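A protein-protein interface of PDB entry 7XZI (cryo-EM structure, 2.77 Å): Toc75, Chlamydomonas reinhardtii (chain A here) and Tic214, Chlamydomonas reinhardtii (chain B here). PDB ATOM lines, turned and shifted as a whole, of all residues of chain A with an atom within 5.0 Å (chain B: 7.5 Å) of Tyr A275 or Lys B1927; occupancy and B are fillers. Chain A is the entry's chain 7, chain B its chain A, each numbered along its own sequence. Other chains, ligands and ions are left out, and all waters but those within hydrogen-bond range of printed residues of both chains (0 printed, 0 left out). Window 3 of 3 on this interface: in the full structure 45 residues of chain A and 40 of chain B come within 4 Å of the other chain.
The backbone NH of Leu B1928 lies within hydrogen-bond range of the side-chain hydroxyl of Tyr A275 (3.0 Å).
CA of Gly A245 touches CD2 of Leu B1928, 3.8 Å away.
Leu B1928 touches Pro A274.
Pro A274 touches Ser B1930 (CG to CA, 3.8 Å).
Tyr A275 touches Lys B1927 (OH to C, 3.9 Å).
Of the printed residues of chain B, Gly A245 touches Leu B1928 (3.8 Å).
Of the printed residues of chain B, Pro A274 touches Leu B1928 and Ser B1930.
Tyr A275 touches just these residues of chain B: Lys B1927 and Leu B1928.
Lys B1927 touches just one residue of chain A: Tyr A275.
Of the printed residues of chain A, Leu B1928 touches Gly A245, Pro A274 and Tyr A275.
Of the printed residues of chain A, Ser B1930 touches Pro A274 (3.8 Å).
The nearest residue of chain B that does not touch Tyr A275 is Lys B1929 (5.2 Å).
The nearest printed residue of chain A that does not touch Ser B1930 is Tyr A275 (5.9 Å).
Hydrophobic or aromatic side chains of chain B that line the printed part of chain A: Leu B1928.
Hydrophobic or aromatic side chains of chain A that line the printed part of chain B: Pro A274 and Tyr A275.
Among the printed residues, 5 pairs touch across the chains.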
ATOM      1  N   PHE A 243      -5.714  -4.427 -17.275  1.00  0.00           N
ATOM      2  CA  PHE A 243      -6.595  -5.049 -16.296  1.00  0.00           C
ATOM      3  C   PHE A 243      -5.741  -5.756 -15.254  1.00  0.00           C
ATOM      4  O   PHE A 243      -4.691  -6.316 -15.587  1.00  0.00           O
ATOM      5  CB  PHE A 243      -7.547  -6.051 -16.953  1.00  0.00           C
ATOM      6  CG  PHE A 243      -8.566  -5.424 -17.857  1.00  0.00           C
ATOM      7  CD1 PHE A 243      -9.548  -4.592 -17.347  1.00  0.00           C
ATOM      8  CD2 PHE A 243      -8.558  -5.687 -19.216  1.00  0.00           C
ATOM      9  CE1 PHE A 243     -10.492  -4.021 -18.177  1.00  0.00           C
ATOM     10  CE2 PHE A 243      -9.499  -5.120 -20.052  1.00  0.00           C
ATOM     11  CZ  PHE A 243     -10.467  -4.284 -19.531  1.00  0.00           C
ATOM     12  N   ARG A 244      -6.189  -5.725 -13.996  1.00  0.00           N
ATOM     13  CA  ARG A 244      -5.428  -6.362 -12.926  1.00  0.00           C
ATOM     14  C   ARG A 244      -5.266  -7.860 -13.158  1.00  0.00           C
ATOM     15  O   ARG A 244      -4.239  -8.437 -12.782  1.00  0.00           O
ATOM     16  CB  ARG A 244      -6.095  -6.098 -11.575  1.00  0.00           C
ATOM     17  CG  ARG A 244      -5.870  -4.694 -11.043  1.00  0.00           C
ATOM     18  CD  ARG A 244      -6.519  -4.506  -9.684  1.00  0.00           C
ATOM     19  NE  ARG A 244      -6.215  -3.197  -9.126  1.00  0.00           N
ATOM     20  CZ  ARG A 244      -6.891  -2.088  -9.407  1.00  0.00           C
ATOM     21  NH1 ARG A 244      -7.926  -2.102 -10.231  1.00  0.00           N
ATOM     22  NH2 ARG A 244      -6.517  -0.941  -8.852  1.00  0.00           N
ATOM     23  N   GLY A 245      -6.258  -8.506 -13.765  1.00  0.00           N
ATOM     24  CA  GLY A 245      -6.121  -9.911 -14.098  1.00  0.00           C
ATOM     25  C   GLY A 245      -7.150 -10.442 -15.075  1.00  0.00           C
ATOM     26  O   GLY A 245      -8.355 -10.248 -14.894  1.00  0.00           O
ATOM     27  N   GLN A 273       0.144 -13.681 -20.486  1.00  0.00           N
ATOM     28  CA  GLN A 273       0.355 -13.554 -19.055  1.00  0.00           C
ATOM     29  C   GLN A 273      -0.966 -13.264 -18.355  1.00  0.00           C
ATOM     30  O   GLN A 273      -1.756 -12.447 -18.848  1.00  0.00           O
ATOM     31  CB  GLN A 273       1.368 -12.434 -18.753  1.00  0.00           C
ATOM     32  CG  GLN A 273       1.677 -12.241 -17.276  1.00  0.00           C
ATOM     33  CD  GLN A 273       2.681 -11.133 -17.032  1.00  0.00           C
ATOM     34  OE1 GLN A 273       3.183 -10.518 -17.973  1.00  0.00           O
ATOM     35  NE2 GLN A 273       2.981 -10.872 -15.765  1.00  0.00           N
ATOM     36  N   PRO A 274      -1.247 -13.904 -17.219  1.00  0.00           N
ATOM     37  CA  PRO A 274      -2.511 -13.669 -16.511  1.00  0.00           C
ATOM     38  C   PRO A 274      -2.534 -12.426 -15.635  1.00  0.00           C
ATOM     39  O   PRO A 274      -3.548 -12.184 -14.973  1.00  0.00           O
ATOM     40  CB  PRO A 274      -2.651 -14.935 -15.655  1.00  0.00           C
ATOM     41  CG  PRO A 274      -1.250 -15.344 -15.379  1.00  0.00           C
ATOM     42  CD  PRO A 274      -0.476 -15.011 -16.626  1.00  0.00           C
ATOM     43  N   TYR A 275      -1.466 -11.632 -15.601  1.00  0.00           N
ATOM     44  CA  TYR A 275      -1.404 -10.436 -14.774  1.00  0.00           C
ATOM     45  C   TYR A 275      -1.107  -9.216 -15.634  1.00  0.00           C
ATOM     46  O   TYR A 275      -0.327  -9.292 -16.589  1.00  0.00           O
ATOM     47  CB  TYR A 275      -0.340 -10.566 -13.678  1.00  0.00           C
ATOM     48  CG  TYR A 275      -0.684 -11.562 -12.592  1.00  0.00           C
ATOM     49  CD1 TYR A 275      -1.679 -11.287 -11.662  1.00  0.00           C
ATOM     50  CD2 TYR A 275      -0.006 -12.767 -12.488  1.00  0.00           C
ATOM     51  CE1 TYR A 275      -1.995 -12.192 -10.665  1.00  0.00           C
ATOM     52  CE2 TYR A 275      -0.314 -13.677 -11.495  1.00  0.00           C
ATOM     53  CZ  TYR A 275      -1.308 -13.384 -10.587  1.00  0.00           C
ATOM     54  OH  TYR A 275      -1.616 -14.289  -9.597  1.00  0.00           O
ATOM     55  N   MET A 276      -1.739  -8.092 -15.281  1.00  0.00           N
ATOM     56  CA  MET A 276      -1.534  -6.811 -15.960  1.00  0.00           C
ATOM     57  C   MET A 276      -1.820  -6.918 -17.457  1.00  0.00           C
ATOM     58  O   MET A 276      -1.041  -6.457 -18.293  1.00  0.00           O
ATOM     59  CB  MET A 276      -0.123  -6.273 -15.710  1.00  0.00           C
ATOM     60  CG  MET A 276       0.299  -6.302 -14.247  1.00  0.00           C
ATOM     61  SD  MET A 276      -0.821  -5.403 -13.154  1.00  0.00           S
ATOM     62  CE  MET A 276      -0.511  -3.714 -13.658  1.00  0.00           C
ATOM     63  N   VAL A 277      -2.952  -7.536 -17.798  1.00  0.00           N
ATOM     64  CA  VAL A 277      -3.327  -7.701 -19.197  1.00  0.00           C
ATOM     65  C   VAL A 277      -3.900  -6.399 -19.736  1.00  0.00           C
ATOM     66  O   VAL A 277      -4.766  -5.772 -19.112  1.00  0.00           O
ATOM     67  CB  VAL A 277      -4.334  -8.853 -19.351  1.00  0.00           C
ATOM     68  CG1 VAL A 277      -4.547  -9.179 -20.822  1.00  0.00           C
ATOM     69  CG2 VAL A 277      -3.863 -10.076 -18.585  1.00  0.00           C
ATOM     70  N   MET B1925      -7.106 -11.640  -1.138  1.00  0.00           N
ATOM     71  CA  MET B1925      -7.174 -11.233  -2.529  1.00  0.00           C
ATOM     72  C   MET B1925      -6.810 -12.458  -3.358  1.00  0.00           C
ATOM     73  O   MET B1925      -5.772 -13.085  -3.088  1.00  0.00           O
ATOM     74  CB  MET B1925      -6.238 -10.069  -2.854  1.00  0.00           C
ATOM     75  CG  MET B1925      -6.362  -9.549  -4.279  1.00  0.00           C
ATOM     76  SD  MET B1925      -5.535  -7.968  -4.536  1.00  0.00           S
ATOM     77  CE  MET B1925      -6.565  -6.882  -3.554  1.00  0.00           C
ATOM     78  N   PRO B1926      -7.627 -12.824  -4.344  1.00  0.00           N
ATOM     79  CA  PRO B1926      -7.396 -14.078  -5.070  1.00  0.00           C
ATOM     80  C   PRO B1926      -6.099 -14.052  -5.865  1.00  0.00           C
ATOM     81  O   PRO B1926      -5.650 -13.003  -6.330  1.00  0.00           O
ATOM     82  CB  PRO B1926      -8.616 -14.182  -5.995  1.00  0.00           C
ATOM     83  CG  PRO B1926      -9.638 -13.273  -5.397  1.00  0.00           C
ATOM     84  CD  PRO B1926      -8.868 -12.156  -4.771  1.00  0.00           C
ATOM     85  N   LYS B1927      -5.500 -15.229  -6.014  1.00  0.00           N
ATOM     86  CA  LYS B1927      -4.333 -15.422  -6.862  1.00  0.00           C
ATOM     87  C   LYS B1927      -4.744 -16.173  -8.122  1.00  0.00           C
ATOM     88  O   LYS B1927      -5.550 -17.106  -8.065  1.00  0.00           O
ATOM     89  CB  LYS B1927      -3.237 -16.194  -6.124  1.00  0.00           C
ATOM     90  N   LEU B1928      -4.185 -15.764  -9.257  1.00  0.00           N
ATOM     91  CA  LEU B1928      -4.563 -16.295 -10.559  1.00  0.00           C
ATOM     92  C   LEU B1928      -3.527 -17.303 -11.036  1.00  0.00           C
ATOM     93  O   LEU B1928      -2.321 -17.051 -10.946  1.00  0.00           O
ATOM     94  CB  LEU B1928      -4.716 -15.171 -11.587  1.00  0.00           C
ATOM     95  CG  LEU B1928      -6.129 -14.629 -11.820  1.00  0.00           C
ATOM     96  CD1 LEU B1928      -6.754 -14.128 -10.526  1.00  0.00           C
ATOM     97  CD2 LEU B1928      -6.111 -13.529 -12.869  1.00  0.00           C
ATOM     98  N   LYS B1929      -4.004 -18.440 -11.536  1.00  0.00           N
ATOM     99  CA  LYS B1929      -3.127 -19.447 -12.113  1.00  0.00           C
ATOM    100  C   LYS B1929      -2.889 -19.153 -13.589  1.00  0.00           C
ATOM    101  O   LYS B1929      -3.793 -18.710 -14.302  1.00  0.00           O
ATOM    102  CB  LYS B1929      -3.729 -20.843 -11.946  1.00  0.00           C
ATOM    103  N   SER B1930      -1.656 -19.395 -14.040  1.00  0.00           N
ATOM    104  CA  SER B1930      -1.314 -19.134 -15.435  1.00  0.00           C
ATOM    105  C   SER B1930      -2.112 -20.027 -16.377  1.00  0.00           C
ATOM    106  O   SER B1930      -2.504 -19.597 -17.469  1.00  0.00           O
ATOM    107  CB  SER B1930       0.185 -19.327 -15.654  1.00  0.00           C
ATOM    108  OG  SER B1930       0.935 -18.406 -14.881  1.00  0.00           O
ATOM    109  N   LEU B1938     -13.994 -17.680  -9.014  1.00  0.00           N
ATOM    110  CA  LEU B1938     -12.881 -17.481  -8.096  1.00  0.00           C
ATOM    111  C   LEU B1938     -13.301 -17.515  -6.633  1.00  0.00           C
ATOM    112  O   LEU B1938     -12.428 -17.461  -5.759  1.00  0.00           O
ATOM    113  CB  LEU B1938     -12.189 -16.148  -8.395  1.00  0.00           C
ATOM    114  CG  LEU B1938     -11.748 -15.923  -9.843  1.00  0.00           C
ATOM    115  CD1 LEU B1938     -11.063 -14.574  -9.994  1.00  0.00           C
ATOM    116  CD2 LEU B1938     -10.838 -17.048 -10.308  1.00  0.00           C
ATOM    117  N   GLN B1940     -14.232 -15.303  -4.997  1.00  0.00           N
ATOM    118  CA  GLN B1940     -13.982 -13.959  -4.476  1.00  0.00           C
ATOM    119  C   GLN B1940     -13.709 -13.051  -5.671  1.00  0.00           C
ATOM    120  O   GLN B1940     -12.665 -13.173  -6.318  1.00  0.00           O
ATOM    121  CB  GLN B1940     -12.821 -13.950  -3.491  1.00  0.00           C
ATOM    122  CG  GLN B1940     -12.501 -12.572  -2.938  1.00  0.00           C
ATOM    123  CD  GLN B1940     -11.342 -12.583  -1.966  1.00  0.00           C
ATOM    124  OE1 GLN B1940     -11.027 -11.566  -1.346  1.00  0.00           O
ATOM    125  NE2 GLN B1940     -10.698 -13.736  -1.827  1.00  0.00           N
